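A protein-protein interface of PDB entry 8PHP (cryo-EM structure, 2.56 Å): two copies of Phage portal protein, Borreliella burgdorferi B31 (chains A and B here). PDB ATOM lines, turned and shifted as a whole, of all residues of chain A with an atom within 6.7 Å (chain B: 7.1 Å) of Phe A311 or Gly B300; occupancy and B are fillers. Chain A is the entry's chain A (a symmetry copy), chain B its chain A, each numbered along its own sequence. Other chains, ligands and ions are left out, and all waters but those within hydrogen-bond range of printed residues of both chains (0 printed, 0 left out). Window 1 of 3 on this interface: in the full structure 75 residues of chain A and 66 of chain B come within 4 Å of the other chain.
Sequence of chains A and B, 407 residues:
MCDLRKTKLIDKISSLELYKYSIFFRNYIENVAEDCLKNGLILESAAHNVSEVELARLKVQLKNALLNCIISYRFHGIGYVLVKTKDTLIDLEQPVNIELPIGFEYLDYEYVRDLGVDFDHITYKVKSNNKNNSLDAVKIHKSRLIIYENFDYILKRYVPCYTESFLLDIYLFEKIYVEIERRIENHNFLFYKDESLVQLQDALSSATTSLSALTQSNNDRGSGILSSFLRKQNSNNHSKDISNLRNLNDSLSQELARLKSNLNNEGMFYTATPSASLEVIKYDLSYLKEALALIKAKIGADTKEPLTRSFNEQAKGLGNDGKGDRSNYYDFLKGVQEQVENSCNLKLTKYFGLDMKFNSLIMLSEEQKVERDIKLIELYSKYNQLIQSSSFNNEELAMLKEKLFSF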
ATOM      1  N   PHE A  24     -11.493  29.229  30.674  1.00  0.00           N
ATOM      2  CA  PHE A  24     -11.156  28.099  31.534  1.00  0.00           C
ATOM      3  C   PHE A  24     -12.305  27.764  32.475  1.00  0.00           C
ATOM      4  O   PHE A  24     -12.609  26.587  32.700  1.00  0.00           O
ATOM      5  CB  PHE A  24      -9.885  28.412  32.324  1.00  0.00           C
ATOM      6  CG  PHE A  24      -9.294  27.225  33.026  1.00  0.00           C
ATOM      7  CD1 PHE A  24      -8.760  26.170  32.306  1.00  0.00           C
ATOM      8  CD2 PHE A  24      -9.265  27.168  34.408  1.00  0.00           C
ATOM      9  CE1 PHE A  24      -8.213  25.080  32.953  1.00  0.00           C
ATOM     10  CE2 PHE A  24      -8.719  26.079  35.060  1.00  0.00           C
ATOM     11  CZ  PHE A  24      -8.193  25.035  34.332  1.00  0.00           C
ATOM     12  N   PHE A 173      -5.465  32.577  38.807  1.00  0.00           N
ATOM     13  CA  PHE A 173      -4.926  32.067  37.552  1.00  0.00           C
ATOM     14  C   PHE A 173      -5.007  33.118  36.453  1.00  0.00           C
ATOM     15  O   PHE A 173      -4.069  33.279  35.663  1.00  0.00           O
ATOM     16  CB  PHE A 173      -5.674  30.798  37.146  1.00  0.00           C
ATOM     17  CG  PHE A 173      -5.068  30.078  35.976  1.00  0.00           C
ATOM     18  CD1 PHE A 173      -3.704  30.132  35.738  1.00  0.00           C
ATOM     19  CD2 PHE A 173      -5.862  29.339  35.115  1.00  0.00           C
ATOM     20  CE1 PHE A 173      -3.148  29.467  34.662  1.00  0.00           C
ATOM     21  CE2 PHE A 173      -5.310  28.672  34.041  1.00  0.00           C
ATOM     22  CZ  PHE A 173      -3.952  28.736  33.813  1.00  0.00           C
ATOM     23  N   LEU A 292       2.135  30.189  39.796  1.00  0.00           N
ATOM     24  CA  LEU A 292       1.448  29.280  38.883  1.00  0.00           C
ATOM     25  C   LEU A 292       1.563  27.835  39.350  1.00  0.00           C
ATOM     26  O   LEU A 292       0.597  27.068  39.262  1.00  0.00           O
ATOM     27  CB  LEU A 292       2.007  29.433  37.469  1.00  0.00           C
ATOM     28  CG  LEU A 292       1.385  28.523  36.408  1.00  0.00           C
ATOM     29  CD1 LEU A 292      -0.124  28.690  36.382  1.00  0.00           C
ATOM     30  CD2 LEU A 292       1.980  28.798  35.039  1.00  0.00           C
ATOM     31  N   ILE A 295      -0.807  27.452  42.241  1.00  0.00           N
ATOM     32  CA  ILE A 295      -2.199  27.524  41.807  1.00  0.00           C
ATOM     33  C   ILE A 295      -2.609  26.237  41.101  1.00  0.00           C
ATOM     34  O   ILE A 295      -3.720  25.731  41.305  1.00  0.00           O
ATOM     35  CB  ILE A 295      -2.412  28.761  40.916  1.00  0.00           C
ATOM     36  CG1 ILE A 295      -2.415  30.031  41.768  1.00  0.00           C
ATOM     37  CG2 ILE A 295      -3.708  28.648  40.133  1.00  0.00           C
ATOM     38  CD1 ILE A 295      -2.128  31.288  40.986  1.00  0.00           C
ATOM     39  N   LYS A 296      -1.725  25.686  40.267  1.00  0.00           N
ATOM     40  CA  LYS A 296      -2.054  24.459  39.547  1.00  0.00           C
ATOM     41  C   LYS A 296      -2.296  23.301  40.508  1.00  0.00           C
ATOM     42  O   LYS A 296      -3.203  22.488  40.294  1.00  0.00           O
ATOM     43  CB  LYS A 296      -0.942  24.112  38.560  1.00  0.00           C
ATOM     44  CG  LYS A 296      -1.286  22.961  37.630  1.00  0.00           C
ATOM     45  CD  LYS A 296      -0.179  22.704  36.624  1.00  0.00           C
ATOM     46  CE  LYS A 296      -0.545  21.566  35.686  1.00  0.00           C
ATOM     47  NZ  LYS A 296       0.589  21.186  34.802  1.00  0.00           N
ATOM     48  N   ILE A 299      -5.771  23.782  42.060  1.00  0.00           N
ATOM     49  CA  ILE A 299      -6.858  23.476  41.135  1.00  0.00           C
ATOM     50  C   ILE A 299      -7.062  21.969  41.032  1.00  0.00           C
ATOM     51  O   ILE A 299      -8.198  21.479  41.037  1.00  0.00           O
ATOM     52  CB  ILE A 299      -6.582  24.109  39.759  1.00  0.00           C
ATOM     53  CG1 ILE A 299      -6.756  25.626  39.829  1.00  0.00           C
ATOM     54  CG2 ILE A 299      -7.501  23.520  38.701  1.00  0.00           C
ATOM     55  CD1 ILE A 299      -6.275  26.353  38.595  1.00  0.00           C
ATOM     56  N   PRO A 306     -10.477  15.563  34.818  1.00  0.00           N
ATOM     57  CA  PRO A 306      -9.060  15.442  34.436  1.00  0.00           C
ATOM     58  C   PRO A 306      -8.550  16.565  33.552  1.00  0.00           C
ATOM     59  O   PRO A 306      -7.375  16.936  33.661  1.00  0.00           O
ATOM     60  CB  PRO A 306      -9.016  14.089  33.712  1.00  0.00           C
ATOM     61  CG  PRO A 306     -10.404  13.900  33.202  1.00  0.00           C
ATOM     62  CD  PRO A 306     -11.291  14.469  34.267  1.00  0.00           C
ATOM     63  N   LEU A 307      -9.389  17.114  32.673  1.00  0.00           N
ATOM     64  CA  LEU A 307      -8.923  18.162  31.772  1.00  0.00           C
ATOM     65  C   LEU A 307      -8.630  19.453  32.527  1.00  0.00           C
ATOM     66  O   LEU A 307      -7.675  20.167  32.198  1.00  0.00           O
ATOM     67  CB  LEU A 307      -9.950  18.405  30.666  1.00  0.00           C
ATOM     68  CG  LEU A 307      -9.815  17.552  29.404  1.00  0.00           C
ATOM     69  CD1 LEU A 307     -10.210  16.109  29.671  1.00  0.00           C
ATOM     70  CD2 LEU A 307     -10.652  18.133  28.278  1.00  0.00           C
ATOM     71  N   THR A 308      -9.440  19.772  33.537  1.00  0.00           N
ATOM     72  CA  THR A 308      -9.217  20.991  34.305  1.00  0.00           C
ATOM     73  C   THR A 308      -7.971  20.879  35.177  1.00  0.00           C
ATOM     74  O   THR A 308      -7.184  21.828  35.268  1.00  0.00           O
ATOM     75  CB  THR A 308     -10.447  21.306  35.157  1.00  0.00           C
ATOM     76  OG1 THR A 308     -11.569  21.552  34.302  1.00  0.00           O
ATOM     77  CG2 THR A 308     -10.203  22.533  36.019  1.00  0.00           C
ATOM     78  N   ARG A 309      -7.773  19.726  35.821  1.00  0.00           N
ATOM     79  CA  ARG A 309      -6.614  19.556  36.693  1.00  0.00           C
ATOM     80  C   ARG A 309      -5.308  19.619  35.911  1.00  0.00           C
ATOM     81  O   ARG A 309      -4.350  20.271  36.341  1.00  0.00           O
ATOM     82  CB  ARG A 309      -6.703  18.229  37.442  1.00  0.00           C
ATOM     83  CG  ARG A 309      -8.019  17.969  38.141  1.00  0.00           C
ATOM     84  CD  ARG A 309      -8.004  16.607  38.818  1.00  0.00           C
ATOM     85  NE  ARG A 309      -7.003  16.536  39.875  1.00  0.00           N
ATOM     86  CZ  ARG A 309      -5.817  15.955  39.748  1.00  0.00           C
ATOM     87  NH1 ARG A 309      -5.452  15.367  38.621  1.00  0.00           N
ATOM     88  NH2 ARG A 309      -4.976  15.965  40.778  1.00  0.00           N
ATOM     89  N   SER A 310      -5.249  18.944  34.768  1.00  0.00           N
ATOM     90  CA  SER A 310      -4.014  18.804  34.010  1.00  0.00           C
ATOM     91  C   SER A 310      -3.824  19.893  32.965  1.00  0.00           C
ATOM     92  O   SER A 310      -2.850  19.834  32.210  1.00  0.00           O
ATOM     93  CB  SER A 310      -3.970  17.433  33.332  1.00  0.00           C
ATOM     94  OG  SER A 310      -5.061  17.275  32.441  1.00  0.00           O
ATOM     95  N   PHE A 311      -4.720  20.879  32.909  1.00  0.00           N
ATOM     96  CA  PHE A 311      -4.676  21.934  31.896  1.00  0.00           C
ATOM     97  C   PHE A 311      -4.716  21.337  30.490  1.00  0.00           C
ATOM     98  O   PHE A 311      -3.898  21.659  29.626  1.00  0.00           O
ATOM     99  CB  PHE A 311      -3.449  22.831  32.080  1.00  0.00           C
ATOM    100  CG  PHE A 311      -3.514  23.711  33.299  1.00  0.00           C
ATOM    101  CD1 PHE A 311      -4.693  23.851  34.010  1.00  0.00           C
ATOM    102  CD2 PHE A 311      -2.393  24.400  33.729  1.00  0.00           C
ATOM    103  CE1 PHE A 311      -4.753  24.659  35.129  1.00  0.00           C
ATOM    104  CE2 PHE A 311      -2.447  25.210  34.848  1.00  0.00           C
ATOM    105  CZ  PHE A 311      -3.629  25.339  35.548  1.00  0.00           C
ATOM    106  N   ASN A 312      -5.679  20.436  30.276  1.00  0.00           N
ATOM    107  CA  ASN A 312      -5.923  19.799  28.981  1.00  0.00           C
ATOM    108  C   ASN A 312      -4.739  18.952  28.520  1.00  0.00           C
ATOM    109  O   ASN A 312      -4.546  18.738  27.321  1.00  0.00           O
ATOM    110  CB  ASN A 312      -6.283  20.831  27.908  1.00  0.00           C
ATOM    111  CG  ASN A 312      -7.636  21.468  28.143  1.00  0.00           C
ATOM    112  OD1 ASN A 312      -8.388  21.049  29.021  1.00  0.00           O
ATOM    113  ND2 ASN A 312      -7.952  22.488  27.356  1.00  0.00           N
ATOM    114  N   GLU A 313      -3.936  18.454  29.462  1.00  0.00           N
ATOM    115  CA  GLU A 313      -2.791  17.620  29.117  1.00  0.00           C
ATOM    116  C   GLU A 313      -3.054  16.130  29.278  1.00  0.00           C
ATOM    117  O   GLU A 313      -2.363  15.326  28.643  1.00  0.00           O
ATOM    118  CB  GLU A 313      -1.576  18.003  29.967  1.00  0.00           C
ATOM    119  CG  GLU A 313      -0.813  19.208  29.450  1.00  0.00           C
ATOM    120  CD  GLU A 313       0.181  19.744  30.460  1.00  0.00           C
ATOM    121  OE1 GLU A 313       0.129  19.315  31.633  1.00  0.00           O
ATOM    122  OE2 GLU A 313       1.016  20.592  30.083  1.00  0.00           O
ATOM    123  N   GLN A 314      -4.022  15.744  30.101  1.00  0.00           N
ATOM    124  CA  GLN A 314      -4.332  14.345  30.349  1.00  0.00           C
ATOM    125  C   GLN A 314      -5.622  13.951  29.642  1.00  0.00           C
ATOM    126  O   GLN A 314      -6.459  14.794  29.309  1.00  0.00           O
ATOM    127  CB  GLN A 314      -4.455  14.068  31.849  1.00  0.00           C
ATOM    128  CG  GLN A 314      -3.127  13.944  32.572  1.00  0.00           C
ATOM    129  CD  GLN A 314      -3.293  13.832  34.072  1.00  0.00           C
ATOM    130  OE1 GLN A 314      -4.409  13.868  34.589  1.00  0.00           O
ATOM    131  NE2 GLN A 314      -2.179  13.696  34.782  1.00  0.00           N
ATOM    132  N   PHE B 166      -8.681  34.676  26.542  1.00  0.00           N
ATOM    133  CA  PHE B 166      -7.948  34.056  25.442  1.00  0.00           C
ATOM    134  C   PHE B 166      -7.298  35.104  24.548  1.00  0.00           C
ATOM    135  O   PHE B 166      -6.168  34.915  24.081  1.00  0.00           O
ATOM    136  CB  PHE B 166      -8.881  33.163  24.626  1.00  0.00           C
ATOM    137  CG  PHE B 166      -8.163  32.255  23.671  1.00  0.00           C
ATOM    138  CD1 PHE B 166      -7.509  31.125  24.128  1.00  0.00           C
ATOM    139  CD2 PHE B 166      -8.137  32.536  22.316  1.00  0.00           C
ATOM    140  CE1 PHE B 166      -6.845  30.290  23.250  1.00  0.00           C
ATOM    141  CE2 PHE B 166      -7.476  31.706  21.435  1.00  0.00           C
ATOM    142  CZ  PHE B 166      -6.829  30.581  21.902  1.00  0.00           C
ATOM    143  N   ILE B 295       2.901  31.818  29.190  1.00  0.00           N
ATOM    144  CA  ILE B 295       1.880  32.020  28.167  1.00  0.00           C
ATOM    145  C   ILE B 295       1.533  30.702  27.485  1.00  0.00           C
ATOM    146  O   ILE B 295       0.360  30.421  27.211  1.00  0.00           O
ATOM    147  CB  ILE B 295       2.347  33.083  27.156  1.00  0.00           C
ATOM    148  CG1 ILE B 295       2.265  34.477  27.781  1.00  0.00           C
ATOM    149  CG2 ILE B 295       1.518  33.025  25.885  1.00  0.00           C
ATOM    150  CD1 ILE B 295       3.129  35.504  27.092  1.00  0.00           C
ATOM    151  N   LYS B 296       2.541  29.873  27.204  1.00  0.00           N
ATOM    152  CA  LYS B 296       2.285  28.598  26.542  1.00  0.00           C
ATOM    153  C   LYS B 296       1.406  27.694  27.398  1.00  0.00           C
ATOM    154  O   LYS B 296       0.521  27.005  26.879  1.00  0.00           O
ATOM    155  CB  LYS B 296       3.603  27.902  26.208  1.00  0.00           C
ATOM    156  CG  LYS B 296       3.441  26.662  25.345  1.00  0.00           C
ATOM    157  CD  LYS B 296       4.782  26.052  24.983  1.00  0.00           C
ATOM    158  CE  LYS B 296       4.605  24.827  24.102  1.00  0.00           C
ATOM    159  NZ  LYS B 296       5.892  24.116  23.873  1.00  0.00           N
ATOM    160  N   ALA B 297       1.643  27.676  28.711  1.00  0.00           N
ATOM    161  CA  ALA B 297       0.803  26.883  29.603  1.00  0.00           C
ATOM    162  C   ALA B 297      -0.636  27.386  29.600  1.00  0.00           C
ATOM    163  O   ALA B 297      -1.580  26.588  29.614  1.00  0.00           O
ATOM    164  CB  ALA B 297       1.375  26.901  31.019  1.00  0.00           C
ATOM    165  N   LYS B 298      -0.820  28.707  29.590  1.00  0.00           N
ATOM    166  CA  LYS B 298      -2.167  29.269  29.573  1.00  0.00           C
ATOM    167  C   LYS B 298      -2.898  28.933  28.278  1.00  0.00           C
ATOM    168  O   LYS B 298      -4.096  28.631  28.296  1.00  0.00           O
ATOM    169  CB  LYS B 298      -2.107  30.782  29.772  1.00  0.00           C
ATOM    170  CG  LYS B 298      -3.463  31.455  29.810  1.00  0.00           C
ATOM    171  CD  LYS B 298      -4.245  31.054  31.044  1.00  0.00           C
ATOM    172  CE  LYS B 298      -5.482  31.916  31.213  1.00  0.00           C
ATOM    173  NZ  LYS B 298      -6.253  31.530  32.425  1.00  0.00           N
ATOM    174  N   ILE B 299      -2.195  28.991  27.144  1.00  0.00           N
ATOM    175  CA  ILE B 299      -2.824  28.686  25.862  1.00  0.00           C
ATOM    176  C   ILE B 299      -3.294  27.237  25.831  1.00  0.00           C
ATOM    177  O   ILE B 299      -4.403  26.938  25.368  1.00  0.00           O
ATOM    178  CB  ILE B 299      -1.856  28.996  24.706  1.00  0.00           C
ATOM    179  CG1 ILE B 299      -1.701  30.508  24.536  1.00  0.00           C
ATOM    180  CG2 ILE B 299      -2.342  28.365  23.412  1.00  0.00           C
ATOM    181  CD1 ILE B 299      -0.592  30.904  23.589  1.00  0.00           C
ATOM    182  N   GLY B 300      -2.466  26.317  26.328  1.00  0.00           N
ATOM    183  CA  GLY B 300      -2.855  24.919  26.354  1.00  0.00           C
ATOM    184  C   GLY B 300      -4.070  24.651  27.219  1.00  0.00           C
ATOM    185  O   GLY B 300      -4.884  23.781  26.899  1.00  0.00           O
ATOM    186  N   ALA B 301      -4.209  25.384  28.324  1.00  0.00           N
ATOM    187  CA  ALA B 301      -5.352  25.204  29.208  1.00  0.00           C
ATOM    188  C   ALA B 301      -6.623  25.849  28.675  1.00  0.00           C
ATOM    189  O   ALA B 301      -7.717  25.483  29.117  1.00  0.00           O
ATOM    190  CB  ALA B 301      -5.038  25.771  30.594  1.00  0.00           C
ATOM    191  N   ASP B 302      -6.510  26.792  27.744  1.00  0.00           N
ATOM    192  CA  ASP B 302      -7.656  27.542  27.249  1.00  0.00           C
ATOM    193  C   ASP B 302      -8.260  26.959  25.978  1.00  0.00           C
ATOM    194  O   ASP B 302      -9.266  27.484  25.494  1.00  0.00           O
ATOM    195  CB  ASP B 302      -7.262  29.001  27.004  1.00  0.00           C
ATOM    196  CG  ASP B 302      -7.250  29.821  28.277  1.00  0.00           C
ATOM    197  OD1 ASP B 302      -7.507  29.249  29.357  1.00  0.00           O
ATOM    198  OD2 ASP B 302      -6.986  31.039  28.199  1.00  0.00           O
ATOM    199  N   THR B 303      -7.682  25.894  25.428  1.00  0.00           N
ATOM    200  CA  THR B 303      -8.200  25.306  24.203  1.00  0.00           C
ATOM    201  C   THR B 303      -7.873  23.821  24.179  1.00  0.00           C
ATOM    202  O   THR B 303      -7.013  23.343  24.922  1.00  0.00           O
ATOM    203  CB  THR B 303      -7.635  25.997  22.955  1.00  0.00           C
ATOM    204  OG1 THR B 303      -8.293  25.492  21.787  1.00  0.00           O
ATOM    205  CG2 THR B 303      -6.142  25.747  22.836  1.00  0.00           C
ATOM    206  N   LYS B 304      -8.581  23.096  23.316  1.00  0.00           N
ATOM    207  CA  LYS B 304      -8.396  21.660  23.164  1.00  0.00           C
ATOM    208  C   LYS B 304      -7.772  21.276  21.830  1.00  0.00           C
ATOM    209  O   LYS B 304      -7.488  20.093  21.615  1.00  0.00           O
ATOM    210  CB  LYS B 304      -9.736  20.934  23.328  1.00  0.00           C
ATOM    211  CG  LYS B 304     -10.224  20.842  24.763  1.00  0.00           C
ATOM    212  CD  LYS B 304     -11.706  20.515  24.815  1.00  0.00           C
ATOM    213  CE  LYS B 304     -12.275  20.751  26.203  1.00  0.00           C
ATOM    214  NZ  LYS B 304     -13.755  20.596  26.228  1.00  0.00           N
ATOM    215  N   GLU B 305      -7.553  22.229  20.936  1.00  0.00           N
ATOM    216  CA  GLU B 305      -6.990  21.916  19.628  1.00  0.00           C
ATOM    217  C   GLU B 305      -5.512  21.583  19.785  1.00  0.00           C
ATOM    218  O   GLU B 305      -4.741  22.436  20.241  1.00  0.00           O
ATOM    219  CB  GLU B 305      -7.188  23.093  18.677  1.00  0.00           C
ATOM    220  CG  GLU B 305      -7.109  22.736  17.202  1.00  0.00           C
ATOM    221  CD  GLU B 305      -5.693  22.741  16.667  1.00  0.00           C
ATOM    222  OE1 GLU B 305      -4.861  23.513  17.189  1.00  0.00           O
ATOM    223  OE2 GLU B 305      -5.413  21.974  15.723  1.00  0.00           O
ATOM    224  N   THR B 308      -2.684  24.051  18.338  1.00  0.00           N
ATOM    225  CA  THR B 308      -2.543  25.345  18.996  1.00  0.00           C
ATOM    226  C   THR B 308      -1.846  25.209  20.346  1.00  0.00           C
ATOM    227  O   THR B 308      -0.983  26.026  20.688  1.00  0.00           O
ATOM    228  CB  THR B 308      -3.914  26.000  19.160  1.00  0.00           C
ATOM    229  OG1 THR B 308      -4.481  26.250  17.868  1.00  0.00           O
ATOM    230  CG2 THR B 308      -3.794  27.316  19.910  1.00  0.00           C
ATOM    231  N   ARG B 309      -2.202  24.182  21.122  1.00  0.00           N
ATOM    232  CA  ARG B 309      -1.594  24.005  22.438  1.00  0.00           C
ATOM    233  C   ARG B 309      -0.102  23.716  22.333  1.00  0.00           C
ATOM    234  O   ARG B 309       0.701  24.282  23.083  1.00  0.00           O
ATOM    235  CB  ARG B 309      -2.286  22.873  23.195  1.00  0.00           C
ATOM    236  CG  ARG B 309      -3.795  22.957  23.241  1.00  0.00           C
ATOM    237  CD  ARG B 309      -4.373  21.763  23.984  1.00  0.00           C
ATOM    238  NE  ARG B 309      -3.959  21.740  25.382  1.00  0.00           N
ATOM    239  CZ  ARG B 309      -2.995  20.969  25.867  1.00  0.00           C
ATOM    240  NH1 ARG B 309      -2.327  20.129  25.095  1.00  0.00           N
ATOM    241  NH2 ARG B 309      -2.693  21.045  27.160  1.00  0.00           N
ATOM    242  N   SER B 310       0.286  22.835  21.416  1.00  0.00           N
ATOM    243  CA  SER B 310       1.660  22.365  21.321  1.00  0.00           C
ATOM    244  C   SER B 310       2.513  23.194  20.373  1.00  0.00           C
ATOM    245  O   SER B 310       3.676  22.843  20.152  1.00  0.00           O
ATOM    246  CB  SER B 310       1.681  20.901  20.878  1.00  0.00           C
ATOM    247  OG  SER B 310       1.069  20.747  19.611  1.00  0.00           O
ATOM    248  N   PHE B 311       1.970  24.277  19.816  1.00  0.00           N
ATOM    249  CA  PHE B 311       2.675  25.102  18.833  1.00  0.00           C
ATOM    250  C   PHE B 311       3.104  24.262  17.630  1.00  0.00           C
ATOM    251  O   PHE B 311       4.260  24.285  17.205  1.00  0.00           O
ATOM    252  CB  PHE B 311       3.873  25.817  19.463  1.00  0.00           C
ATOM    253  CG  PHE B 311       3.493  26.912  20.423  1.00  0.00           C
ATOM    254  CD1 PHE B 311       2.188  27.365  20.503  1.00  0.00           C
ATOM    255  CD2 PHE B 311       4.447  27.488  21.244  1.00  0.00           C
ATOM    256  CE1 PHE B 311       1.840  28.369  21.384  1.00  0.00           C
ATOM    257  CE2 PHE B 311       4.105  28.494  22.128  1.00  0.00           C
ATOM    258  CZ  PHE B 311       2.799  28.934  22.197  1.00  0.00           C
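The backbone carbonyl oxygen (O) of Gly B300 sits at hydrogen-bond distance from the side-chain amide nitrogen (ND2) of Asn A312, 3.4 Å away.
The side-chain amide nitrogen (ND2) of Asn A312 sits at hydrogen-bond distance from the backbone carbonyl oxygen (O) of Ala B301 (3.5 Å).
The side-chain amide nitrogen of Asn A312 lies within hydrogen-bond range of the backbone carbonyl oxygen of Thr B303 (2.7 Å).
The guanidinium group (NH2) of Arg B309 lies within hydrogen-bond range of the backbone carbonyl oxygen (O) of Phe A311 (2.8 Å).
O of Asn A312 sits at hydrogen-bond distance from NH2 of Arg B309, 3.0 Å away.
The guanidinium group of Arg B309 is in hydrogen-bond range of the backbone carbonyl oxygen of Gly B300, at 2.7 Å.
The side-chain hydroxyl (OG1) of Thr B303 sits at hydrogen-bond distance from the backbone NH (N) of Glu B305 (3.5 Å).
O of Thr B303 lies close to NE of Arg B309, at 3.5 Å.
NZ of Lys A296 lies within salt-bridge range of OE1 of Glu A313 (3.7 Å).
The backbone carbonyl oxygen (O) of Leu A307 lies within hydrogen-bond range of the backbone NH (N) of Asn A312, at 2.8 Å.
OG of Ser A310 sits at hydrogen-bond distance from N of Glu A313.
Among the printed residues, pairs that only touch across the chains: Phe A24 with Ala B301 (3.4 Å), Phe A24 with Asp B302 (3.9 Å), Phe A173 with Lys B298 (3.4 Å), Leu A307 with Lys B304 (3.7 Å), Phe A311 with Gly B300 (3.6 Å), Phe A311 with Ala B301 (3.7 Å), Asn A312 with Lys B304 (3.8 Å) and Glu A313 with Arg B309 (3.5 Å).
Of the printed residues of chain B, Phe A24 touches Ala B301 (3.4 Å) and Asp B302 (3.9 Å).
Printed residues of chain B within 4 Å of Leu A307: Lys B304 (3.7 Å).
Printed residues of chain B within 4 Å of Phe A311: Gly B300 (3.6 Å), Ala B301 (3.7 Å) and Arg B309 (2.8 Å).
Printed residues of chain B within 4 Å of Glu A313: Arg B309 (3.5 Å).
Gly B300 touches just these residues of chain A: Phe A311 and Asn A312.
Of the printed residues of chain A, Ala B301 touches Phe A24, Phe A311 and Asn A312.
Printed residues of chain A within 4 Å of Thr B303: Asn A312.
Phe B311 touches none of the printed residues of chain A.
The nearest printed residue of chain A that does not touch Lys B304 is Phe A311 (7.9 Å).
Printed residues of chain B that touch a printed residue of chain A: Lys B298, Gly B300, Ala B301, Asp B302, Thr B303, Lys B304 and Arg B309.
Hydrophobic or aromatic side chains of chain B that line the printed part of chain A: Ala B301.
Of the 15 printed residues of chain A, 6 touch a printed residue of chain B.
Printed residues of chain A that touch a printed residue of chain B: Phe A24, Phe A173, Leu A307, Phe A311, Asn A312 and Glu A313.
Hydrophobic or aromatic side chains of chain A that line the printed part of chain B: Phe A24, Phe A173, Leu A307 and Phe A311.
Among the printed residues, 13 pairs touch across the chains.
Among the printed residues, no Asp or Glu carboxylate lies within 4 Å of a Lys or Arg side-chain nitrogen of the other chain.
Phe A311 touches Arg B309, but with the chains exchanged Arg A309 does not touch Phe B311 (18.1 Å).
7 positions are printed for both chains.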
